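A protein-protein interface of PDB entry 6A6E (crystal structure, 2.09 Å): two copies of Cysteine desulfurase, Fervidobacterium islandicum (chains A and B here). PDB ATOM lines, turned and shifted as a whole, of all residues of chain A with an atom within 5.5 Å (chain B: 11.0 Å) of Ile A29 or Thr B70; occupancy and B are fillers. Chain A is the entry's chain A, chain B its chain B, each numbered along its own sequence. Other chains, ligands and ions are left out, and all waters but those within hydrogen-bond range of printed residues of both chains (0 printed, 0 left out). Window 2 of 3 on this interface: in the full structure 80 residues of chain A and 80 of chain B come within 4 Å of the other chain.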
ATOM      1  N   ARG A  27     -15.156 -33.174   9.685  1.00  0.00           N
ATOM      2  CA  ARG A  27     -15.311 -32.996  11.108  1.00  0.00           C
ATOM      3  C   ARG A  27     -16.839 -33.131  11.396  1.00  0.00           C
ATOM      4  O   ARG A  27     -17.663 -32.660  10.614  1.00  0.00           O
ATOM      5  CB  ARG A  27     -14.825 -31.608  11.580  1.00  0.00           C
ATOM      6  CG  ARG A  27     -13.303 -31.365  11.809  1.00  0.00           C
ATOM      7  CD  ARG A  27     -12.717 -32.093  12.998  1.00  0.00           C
ATOM      8  NE  ARG A  27     -13.384 -31.735  14.266  1.00  0.00           N
ATOM      9  CZ  ARG A  27     -13.099 -30.664  15.015  1.00  0.00           C
ATOM     10  NH1 ARG A  27     -12.151 -29.801  14.665  1.00  0.00           N
ATOM     11  NH2 ARG A  27     -13.740 -30.459  16.140  1.00  0.00           N
ATOM     12  N   ASN A  28     -17.191 -33.724  12.536  1.00  0.00           N
ATOM     13  CA  ASN A  28     -18.582 -33.710  13.022  1.00  0.00           C
ATOM     14  C   ASN A  28     -18.649 -32.955  14.331  1.00  0.00           C
ATOM     15  O   ASN A  28     -17.762 -33.126  15.185  1.00  0.00           O
ATOM     16  CB  ASN A  28     -19.096 -35.146  13.253  1.00  0.00           C
ATOM     17  CG  ASN A  28     -19.169 -35.953  11.966  1.00  0.00           C
ATOM     18  OD1 ASN A  28     -19.741 -35.513  10.963  1.00  0.00           O
ATOM     19  ND2 ASN A  28     -18.550 -37.124  11.974  1.00  0.00           N
ATOM     20  N   ILE A  29     -19.723 -32.185  14.506  1.00  0.00           N
ATOM     21  CA  ILE A  29     -20.029 -31.485  15.772  1.00  0.00           C
ATOM     22  C   ILE A  29     -21.299 -32.127  16.327  1.00  0.00           C
ATOM     23  O   ILE A  29     -22.378 -32.023  15.717  1.00  0.00           O
ATOM     24  CB  ILE A  29     -20.333 -29.977  15.555  1.00  0.00           C
ATOM     25  CG1 ILE A  29     -19.380 -29.280  14.552  1.00  0.00           C
ATOM     26  CG2 ILE A  29     -20.392 -29.240  16.875  1.00  0.00           C
ATOM     27  CD1 ILE A  29     -17.924 -29.527  14.787  1.00  0.00           C
ATOM     28  N   ASN A  30     -21.184 -32.785  17.473  1.00  0.00           N
ATOM     29  CA  ASN A  30     -22.287 -33.519  18.055  1.00  0.00           C
ATOM     30  C   ASN A  30     -22.984 -34.431  17.105  1.00  0.00           C
ATOM     31  O   ASN A  30     -24.183 -34.479  17.105  1.00  0.00           O
ATOM     32  CB  ASN A  30     -23.293 -32.541  18.658  1.00  0.00           C
ATOM     33  CG  ASN A  30     -22.692 -31.830  19.811  1.00  0.00           C
ATOM     34  OD1 ASN A  30     -22.040 -32.498  20.627  1.00  0.00           O
ATOM     35  ND2 ASN A  30     -22.781 -30.483  19.848  1.00  0.00           N
ATOM     36  N   GLY A  31     -22.240 -35.138  16.272  1.00  0.00           N
ATOM     37  CA  GLY A  31     -22.828 -36.039  15.307  1.00  0.00           C
ATOM     38  C   GLY A  31     -23.402 -35.442  14.041  1.00  0.00           C
ATOM     39  O   GLY A  31     -23.967 -36.182  13.259  1.00  0.00           O
ATOM     40  N   LYS A  32     -23.257 -34.135  13.810  1.00  0.00           N
ATOM     41  CA  LYS A  32     -23.619 -33.529  12.513  1.00  0.00           C
ATOM     42  C   LYS A  32     -22.368 -32.986  11.767  1.00  0.00           C
ATOM     43  O   LYS A  32     -21.436 -32.425  12.389  1.00  0.00           O
ATOM     44  CB  LYS A  32     -24.612 -32.414  12.714  1.00  0.00           C
ATOM     45  CG  LYS A  32     -25.857 -32.884  13.427  1.00  0.00           C
ATOM     46  CD  LYS A  32     -26.916 -31.847  13.372  1.00  0.00           C
ATOM     47  CE  LYS A  32     -28.209 -32.365  13.995  1.00  0.00           C
ATOM     48  NZ  LYS A  32     -29.298 -31.504  13.460  1.00  0.00           N
ATOM     49  N   ARG A  33     -22.351 -33.157  10.451  1.00  0.00           N
ATOM     50  CA  ARG A  33     -21.225 -32.703   9.678  1.00  0.00           C
ATOM     51  C   ARG A  33     -21.095 -31.177   9.806  1.00  0.00           C
ATOM     52  O   ARG A  33     -22.084 -30.428   9.996  1.00  0.00           O
ATOM     53  CB  ARG A  33     -21.325 -33.115   8.205  1.00  0.00           C
ATOM     54  CG  ARG A  33     -22.360 -32.324   7.428  1.00  0.00           C
ATOM     55  CD  ARG A  33     -22.537 -32.787   5.981  1.00  0.00           C
ATOM     56  NE  ARG A  33     -23.549 -31.965   5.310  1.00  0.00           N
ATOM     57  CZ  ARG A  33     -23.325 -30.802   4.721  1.00  0.00           C
ATOM     58  NH1 ARG A  33     -22.078 -30.306   4.652  1.00  0.00           N
ATOM     59  NH2 ARG A  33     -24.343 -30.120   4.185  1.00  0.00           N
ATOM     60  N   LEU A  34     -19.843 -30.755   9.696  1.00  0.00           N
ATOM     61  CA  LEU A  34     -19.479 -29.343   9.746  1.00  0.00           C
ATOM     62  C   LEU A  34     -20.079 -28.658   8.561  1.00  0.00           C
ATOM     63  O   LEU A  34     -19.858 -29.023   7.416  1.00  0.00           O
ATOM     64  CB  LEU A  34     -17.937 -29.166   9.773  1.00  0.00           C
ATOM     65  CG  LEU A  34     -17.473 -27.706   9.549  1.00  0.00           C
ATOM     66  CD1 LEU A  34     -17.954 -26.811  10.712  1.00  0.00           C
ATOM     67  CD2 LEU A  34     -15.965 -27.650   9.377  1.00  0.00           C
ATOM     68  N   ASP A 363     -24.318 -23.790  15.909  1.00  0.00           N
ATOM     69  CA  ASP A 363     -23.102 -24.588  16.075  1.00  0.00           C
ATOM     70  C   ASP A 363     -23.287 -25.909  16.905  1.00  0.00           C
ATOM     71  O   ASP A 363     -22.884 -26.998  16.484  1.00  0.00           O
ATOM     72  CB  ASP A 363     -21.982 -23.722  16.730  1.00  0.00           C
ATOM     73  CG  ASP A 363     -20.767 -24.551  17.162  1.00  0.00           C
ATOM     74  OD1 ASP A 363     -20.046 -25.167  16.341  1.00  0.00           O
ATOM     75  OD2 ASP A 363     -20.512 -24.601  18.365  1.00  0.00           O
ATOM     76  N   GLU A 364     -23.901 -25.817  18.073  1.00  0.00           N
ATOM     77  CA  GLU A 364     -23.952 -26.992  18.933  1.00  0.00           C
ATOM     78  C   GLU A 364     -24.965 -28.027  18.377  1.00  0.00           C
ATOM     79  O   GLU A 364     -24.659 -29.220  18.285  1.00  0.00           O
ATOM     80  CB  GLU A 364     -24.278 -26.592  20.357  1.00  0.00           C
ATOM     81  CG  GLU A 364     -23.536 -27.454  21.363  1.00  0.00           C
ATOM     82  CD  GLU A 364     -24.213 -27.429  22.699  1.00  0.00           C
ATOM     83  OE1 GLU A 364     -25.018 -28.354  22.933  1.00  0.00           O
ATOM     84  OE2 GLU A 364     -23.954 -26.479  23.502  1.00  0.00           O
ATOM     85  N   GLY A 367     -24.222 -28.056  13.782  1.00  0.00           N
ATOM     86  CA  GLY A 367     -22.849 -28.098  13.226  1.00  0.00           C
ATOM     87  C   GLY A 367     -22.486 -26.937  12.273  1.00  0.00           C
ATOM     88  O   GLY A 367     -21.487 -27.002  11.545  1.00  0.00           O
ATOM     89  N   PHE B  56      -3.138 -28.582  12.379  1.00  0.00           N
ATOM     90  CA  PHE B  56      -3.856 -27.369  12.777  1.00  0.00           C
ATOM     91  C   PHE B  56      -4.553 -26.759  11.596  1.00  0.00           C
ATOM     92  O   PHE B  56      -5.722 -26.480  11.666  1.00  0.00           O
ATOM     93  CB  PHE B  56      -2.915 -26.388  13.504  1.00  0.00           C
ATOM     94  CG  PHE B  56      -3.572 -25.149  13.930  1.00  0.00           C
ATOM     95  CD1 PHE B  56      -4.340 -25.145  15.086  1.00  0.00           C
ATOM     96  CD2 PHE B  56      -3.517 -24.012  13.166  1.00  0.00           C
ATOM     97  CE1 PHE B  56      -5.019 -24.025  15.451  1.00  0.00           C
ATOM     98  CE2 PHE B  56      -4.166 -22.848  13.560  1.00  0.00           C
ATOM     99  CZ  PHE B  56      -4.925 -22.852  14.706  1.00  0.00           C
ATOM    100  N   TYR B  59      -7.513 -29.150  10.262  1.00  0.00           N
ATOM    101  CA  TYR B  59      -8.532 -29.703  11.134  1.00  0.00           C
ATOM    102  C   TYR B  59      -8.956 -28.827  12.299  1.00  0.00           C
ATOM    103  O   TYR B  59      -9.985 -29.106  12.864  1.00  0.00           O
ATOM    104  CB  TYR B  59      -8.134 -31.085  11.668  1.00  0.00           C
ATOM    105  CG  TYR B  59      -8.037 -32.177  10.661  1.00  0.00           C
ATOM    106  CD1 TYR B  59      -9.180 -32.747  10.091  1.00  0.00           C
ATOM    107  CD2 TYR B  59      -6.786 -32.671  10.268  1.00  0.00           C
ATOM    108  CE1 TYR B  59      -9.081 -33.790   9.167  1.00  0.00           C
ATOM    109  CE2 TYR B  59      -6.675 -33.682   9.354  1.00  0.00           C
ATOM    110  CZ  TYR B  59      -7.824 -34.225   8.814  1.00  0.00           C
ATOM    111  OH  TYR B  59      -7.672 -35.172   7.884  1.00  0.00           O
ATOM    112  N   HIS B  60      -8.240 -27.754  12.652  1.00  0.00           N
ATOM    113  CA  HIS B  60      -8.599 -26.985  13.830  1.00  0.00           C
ATOM    114  C   HIS B  60      -8.517 -25.467  13.553  1.00  0.00           C
ATOM    115  O   HIS B  60      -8.288 -24.668  14.457  1.00  0.00           O
ATOM    116  CB  HIS B  60      -7.647 -27.348  14.985  1.00  0.00           C
ATOM    117  CG  HIS B  60      -7.688 -28.806  15.321  1.00  0.00           C
ATOM    118  ND1 HIS B  60      -8.755 -29.371  16.002  1.00  0.00           N
ATOM    119  CD2 HIS B  60      -6.859 -29.830  14.986  1.00  0.00           C
ATOM    120  CE1 HIS B  60      -8.564 -30.681  16.095  1.00  0.00           C
ATOM    121  NE2 HIS B  60      -7.437 -30.988  15.461  1.00  0.00           N
ATOM    122  N   TYR B  61      -8.769 -25.102  12.328  1.00  0.00           N
ATOM    123  CA  TYR B  61      -8.530 -23.752  11.847  1.00  0.00           C
ATOM    124  C   TYR B  61      -9.784 -22.884  11.724  1.00  0.00           C
ATOM    125  O   TYR B  61     -10.777 -23.364  11.267  1.00  0.00           O
ATOM    126  CB  TYR B  61      -7.812 -23.810  10.489  1.00  0.00           C
ATOM    127  CG  TYR B  61      -7.560 -22.425   9.978  1.00  0.00           C
ATOM    128  CD1 TYR B  61      -6.455 -21.717  10.388  1.00  0.00           C
ATOM    129  CD2 TYR B  61      -8.434 -21.819   9.126  1.00  0.00           C
ATOM    130  CE1 TYR B  61      -6.257 -20.443   9.963  1.00  0.00           C
ATOM    131  CE2 TYR B  61      -8.254 -20.538   8.717  1.00  0.00           C
ATOM    132  CZ  TYR B  61      -7.159 -19.859   9.116  1.00  0.00           C
ATOM    133  OH  TYR B  61      -6.965 -18.593   8.687  1.00  0.00           O
ATOM    134  N   SER B  62      -9.699 -21.640  12.213  1.00  0.00           N
ATOM    135  CA  SER B  62     -10.640 -20.581  12.001  1.00  0.00           C
ATOM    136  C   SER B  62     -10.039 -19.293  12.530  1.00  0.00           C
ATOM    137  O   SER B  62      -8.992 -19.295  13.149  1.00  0.00           O
ATOM    138  CB  SER B  62     -12.014 -20.826  12.695  1.00  0.00           C
ATOM    139  OG  SER B  62     -12.888 -21.612  11.848  1.00  0.00           O
ATOM    140  N   ASN B  63     -10.718 -18.185  12.321  1.00  0.00           N
ATOM    141  CA  ASN B  63     -10.264 -16.927  12.925  1.00  0.00           C
ATOM    142  C   ASN B  63     -10.632 -16.925  14.449  1.00  0.00           C
ATOM    143  O   ASN B  63     -11.504 -17.697  14.875  1.00  0.00           O
ATOM    144  CB  ASN B  63     -10.806 -15.705  12.165  1.00  0.00           C
ATOM    145  CG  ASN B  63      -9.806 -14.541  12.169  1.00  0.00           C
ATOM    146  OD1 ASN B  63      -8.988 -14.456  13.097  1.00  0.00           O
ATOM    147  ND2 ASN B  63      -9.806 -13.701  11.112  1.00  0.00           N
ATOM    148  N   ILE B  64      -9.958 -16.082  15.229  1.00  0.00           N
ATOM    149  CA  ILE B  64      -9.824 -16.259  16.632  1.00  0.00           C
ATOM    150  C   ILE B  64     -10.294 -15.111  17.509  1.00  0.00           C
ATOM    151  O   ILE B  64     -10.524 -13.985  17.027  1.00  0.00           O
ATOM    152  CB  ILE B  64      -8.355 -16.615  17.002  1.00  0.00           C
ATOM    153  CG1 ILE B  64      -7.388 -15.481  16.608  1.00  0.00           C
ATOM    154  CG2 ILE B  64      -8.028 -18.005  16.418  1.00  0.00           C
ATOM    155  CD1 ILE B  64      -5.946 -15.691  17.069  1.00  0.00           C
ATOM    156  N   HIS B  65     -10.383 -15.403  18.800  1.00  0.00           N
ATOM    157  CA  HIS B  65     -10.682 -14.446  19.847  1.00  0.00           C
ATOM    158  C   HIS B  65     -12.167 -14.161  20.083  1.00  0.00           C
ATOM    159  O   HIS B  65     -12.481 -13.378  21.017  1.00  0.00           O
ATOM    160  CB  HIS B  65      -9.895 -13.079  19.757  1.00  0.00           C
ATOM    161  CG  HIS B  65      -8.417 -13.245  19.956  1.00  0.00           C
ATOM    162  ND1 HIS B  65      -7.499 -12.806  19.025  1.00  0.00           N
ATOM    163  CD2 HIS B  65      -7.719 -13.896  20.911  1.00  0.00           C
ATOM    164  CE1 HIS B  65      -6.284 -13.141  19.451  1.00  0.00           C
ATOM    165  NE2 HIS B  65      -6.392 -13.769  20.603  1.00  0.00           N
ATOM    166  N   ARG B  66     -13.044 -14.824  19.332  1.00  0.00           N
ATOM    167  CA  ARG B  66     -14.529 -14.763  19.600  1.00  0.00           C
ATOM    168  C   ARG B  66     -15.044 -16.192  19.632  1.00  0.00           C
ATOM    169  O   ARG B  66     -14.806 -17.009  18.690  1.00  0.00           O
ATOM    170  CB  ARG B  66     -15.256 -14.000  18.497  1.00  0.00           C
ATOM    171  CG  ARG B  66     -14.760 -12.559  18.341  1.00  0.00           C
ATOM    172  CD  ARG B  66     -15.079 -11.815  19.637  1.00  0.00           C
ATOM    173  NE  ARG B  66     -14.663 -10.427  19.559  1.00  0.00           N
ATOM    174  CZ  ARG B  66     -13.480  -9.909  19.902  1.00  0.00           C
ATOM    175  NH1 ARG B  66     -13.306  -8.578  19.778  1.00  0.00           N
ATOM    176  NH2 ARG B  66     -12.473 -10.654  20.368  1.00  0.00           N
ATOM    177  N   ALA B  67     -15.661 -16.525  20.747  1.00  0.00           N
ATOM    178  CA  ALA B  67     -16.147 -17.902  20.981  1.00  0.00           C
ATOM    179  C   ALA B  67     -17.497 -18.118  20.233  1.00  0.00           C
ATOM    180  O   ALA B  67     -18.568 -18.256  20.858  1.00  0.00           O
ATOM    181  CB  ALA B  67     -16.264 -18.152  22.489  1.00  0.00           C
ATOM    182  N   VAL B  68     -17.466 -18.140  18.895  1.00  0.00           N
ATOM    183  CA  VAL B  68     -18.725 -18.112  18.123  1.00  0.00           C
ATOM    184  C   VAL B  68     -19.064 -19.484  17.504  1.00  0.00           C
ATOM    185  O   VAL B  68     -20.203 -19.736  17.130  1.00  0.00           O
ATOM    186  CB  VAL B  68     -18.671 -17.059  16.989  1.00  0.00           C
ATOM    187  CG1 VAL B  68     -18.830 -15.641  17.538  1.00  0.00           C
ATOM    188  CG2 VAL B  68     -17.357 -17.185  16.165  1.00  0.00           C
ATOM    189  N   HIS B  69     -18.084 -20.368  17.364  1.00  0.00           N
ATOM    190  CA  HIS B  69     -18.344 -21.722  16.902  1.00  0.00           C
ATOM    191  C   HIS B  69     -17.202 -22.597  17.285  1.00  0.00           C
ATOM    192  O   HIS B  69     -16.181 -22.124  17.849  1.00  0.00           O
ATOM    193  CB  HIS B  69     -18.699 -21.728  15.400  1.00  0.00           C
ATOM    194  CG  HIS B  69     -17.676 -21.091  14.505  1.00  0.00           C
ATOM    195  ND1 HIS B  69     -16.511 -21.733  14.160  1.00  0.00           N
ATOM    196  CD2 HIS B  69     -17.683 -19.921  13.822  1.00  0.00           C
ATOM    197  CE1 HIS B  69     -15.830 -20.962  13.326  1.00  0.00           C
ATOM    198  NE2 HIS B  69     -16.501 -19.839  13.133  1.00  0.00           N
ATOM    199  N   THR B  70     -17.371 -23.890  17.051  1.00  0.00           N
ATOM    200  CA  THR B  70     -16.453 -24.865  17.527  1.00  0.00           C
ATOM    201  C   THR B  70     -14.979 -24.683  17.022  1.00  0.00           C
ATOM    202  O   THR B  70     -14.064 -24.668  17.830  1.00  0.00           O
ATOM    203  CB  THR B  70     -16.991 -26.306  17.179  1.00  0.00           C
ATOM    204  OG1 THR B  70     -18.194 -26.559  17.933  1.00  0.00           O
ATOM    205  CG2 THR B  70     -15.953 -27.383  17.554  1.00  0.00           C
ATOM    206  N   LEU B  71     -14.760 -24.554  15.722  1.00  0.00           N
ATOM    207  CA  LEU B  71     -13.393 -24.368  15.224  1.00  0.00           C
ATOM    208  C   LEU B  71     -12.797 -23.056  15.696  1.00  0.00           C
ATOM    209  O   LEU B  71     -11.656 -23.028  15.991  1.00  0.00           O
ATOM    210  CB  LEU B  71     -13.344 -24.413  13.728  1.00  0.00           C
ATOM    211  CG  LEU B  71     -13.617 -25.751  13.121  1.00  0.00           C
ATOM    212  CD1 LEU B  71     -13.897 -25.622  11.625  1.00  0.00           C
ATOM    213  CD2 LEU B  71     -12.480 -26.712  13.307  1.00  0.00           C
ATOM    214  N   ALA B  72     -13.589 -21.989  15.796  1.00  0.00           N
ATOM    215  CA  ALA B  72     -13.113 -20.670  16.340  1.00  0.00           C
ATOM    216  C   ALA B  72     -12.548 -20.738  17.760  1.00  0.00           C
ATOM    217  O   ALA B  72     -11.558 -20.099  18.077  1.00  0.00           O
ATOM    218  CB  ALA B  72     -14.222 -19.646  16.282  1.00  0.00           C
ATOM    219  N   SER B  73     -13.233 -21.486  18.626  1.00  0.00           N
ATOM    220  CA  SER B  73     -12.745 -21.764  19.980  1.00  0.00           C
ATOM    221  C   SER B  73     -11.550 -22.612  20.006  1.00  0.00           C
ATOM    222  O   SER B  73     -10.647 -22.309  20.745  1.00  0.00           O
ATOM    223  CB  SER B  73     -13.823 -22.397  20.872  1.00  0.00           C
ATOM    224  OG  SER B  73     -14.891 -21.479  20.912  1.00  0.00           O
ATOM    225  N   GLU B  74     -11.517 -23.672  19.203  1.00  0.00           N
ATOM    226  CA  GLU B  74     -10.320 -24.464  19.126  1.00  0.00           C
ATOM    227  C   GLU B  74      -9.085 -23.618  18.696  1.00  0.00           C
ATOM    228  O   GLU B  74      -8.033 -23.741  19.268  1.00  0.00           O
ATOM    229  CB  GLU B  74     -10.496 -25.658  18.172  1.00  0.00           C
ATOM    230  CG  GLU B  74     -11.416 -26.748  18.736  1.00  0.00           C
ATOM    231  CD  GLU B  74     -11.653 -27.897  17.762  1.00  0.00           C
ATOM    232  OE1 GLU B  74     -10.996 -27.983  16.694  1.00  0.00           O
ATOM    233  OE2 GLU B  74     -12.527 -28.727  18.066  1.00  0.00           O
ATOM    234  N   ALA B  75      -9.237 -22.853  17.644  1.00  0.00           N
ATOM    235  CA  ALA B  75      -8.154 -22.119  17.097  1.00  0.00           C
ATOM    236  C   ALA B  75      -7.694 -21.081  18.112  1.00  0.00           C
ATOM    237  O   ALA B  75      -6.506 -20.874  18.222  1.00  0.00           O
ATOM    238  CB  ALA B  75      -8.566 -21.462  15.793  1.00  0.00           C
ATOM    239  N   THR B  76      -8.643 -20.447  18.839  1.00  0.00           N
ATOM    240  CA  THR B  76      -8.307 -19.455  19.853  1.00  0.00           C
ATOM    241  C   THR B  76      -7.500 -20.040  20.958  1.00  0.00           C
ATOM    242  O   THR B  76      -6.468 -19.447  21.408  1.00  0.00           O
ATOM    243  CB  THR B  76      -9.587 -18.776  20.392  1.00  0.00           C
ATOM    244  OG1 THR B  76     -10.306 -18.190  19.289  1.00  0.00           O
ATOM    245  CG2 THR B  76      -9.234 -17.687  21.320  1.00  0.00           C
ATOM    246  N   VAL B  77      -7.949 -21.187  21.463  1.00  0.00           N
ATOM    247  CA  VAL B  77      -7.215 -21.853  22.531  1.00  0.00           C
ATOM    248  C   VAL B  77      -5.827 -22.233  22.072  1.00  0.00           C
ATOM    249  O   VAL B  77      -4.867 -22.041  22.759  1.00  0.00           O
ATOM    250  CB  VAL B  77      -7.984 -23.076  23.071  1.00  0.00           C
ATOM    251  CG1 VAL B  77      -7.130 -23.866  24.069  1.00  0.00           C
ATOM    252  CG2 VAL B  77      -9.274 -22.603  23.741  1.00  0.00           C
ATOM    253  N   ALA B  78      -5.706 -22.763  20.886  1.00  0.00           N
ATOM    254  CA  ALA B  78      -4.356 -23.170  20.426  1.00  0.00           C
ATOM    255  C   ALA B  78      -3.362 -21.968  20.327  1.00  0.00           C
ATOM    256  O   ALA B  78      -2.192 -22.056  20.726  1.00  0.00           O
ATOM    257  CB  ALA B  78      -4.468 -23.898  19.116  1.00  0.00           C
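Among the printed residues, merely in contact across the chains: Arg A27 with Leu B71 (3.4 Å), Ile A29 with Thr B70 (3.6 Å), Leu A34 with Leu B71 (3.7 Å), Arg A27 with His B60 (3.7 Å) and Asp A363 with His B69 (3.7 Å).
Of the 21 printed residues of chain B, 6 touch a printed residue of chain A.
Printed residues of chain B that touch a printed residue of chain A: Tyr B59, His B60, His B69, Thr B70, Leu B71 and Glu B74.
Hydrophobic or aromatic side chains of chain B that line the printed part of chain A: His B60, His B69 and Leu B71.
Among the printed residues, 8 pairs touch across the chains.
The guanidinium group (NH1) of Arg A27 lies within hydrogen-bond range of the backbone carbonyl oxygen (O) of Tyr B59.
The side-chain carboxylate (OE2) of Glu B74 lies within salt-bridge range of the guanidinium group (NH2) of Arg A27 (2.9 Å).
The side-chain carboxylate (OD1) of Asp A363 lies within hydrogen-bond range of the side-chain hydroxyl (OG1) of Thr B70, at 2.8 Å.
The backbone NH (N) of Leu A34 lies within hydrogen-bond range of the backbone carbonyl oxygen (O) of Arg A27 (3.0 Å).
A ring nitrogen (ND1) of His B60 lies within hydrogen-bond range of the side-chain carboxylate (OE1) of Glu B74, 2.7 Å away.
N of Ala B72 sits at hydrogen-bond distance from ND1 of His B69 (3.4 Å).
The side-chain hydroxyl (OG) of Ser B73 lies within hydrogen-bond range of the backbone carbonyl oxygen (O) of His B69.
No position is printed for both chains.
Of the 8 pairs that touch across the chains among the printed residues, none has its exchanged pair printed and touching as well.
Arg A27 touches just these residues of chain B: Tyr B59, His B60, Leu B71 and Glu B74.
No residue of chain B comes within 4 Å of Asn A28.
Ile A29 touches just one residue of chain B: Thr B70 (3.6 Å).
No residue of chain B comes within 4 Å of Gly A31.
Of the printed residues of chain B, Leu A34 touches Leu B71.
Thr B70 touches just these residues of chain A: Ile A29 and Asp A363.
Of the printed residues of chain A, Leu B71 touches Arg A27 (3.4 Å) and Leu A34 (3.7 Å).
Thr B76 touches none of the printed residues of chain A.
Ala B78 touches none of the printed residues of chain A.
The nearest residue of chain B that does not touch Ile A29 is Leu B71 (6.0 Å).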
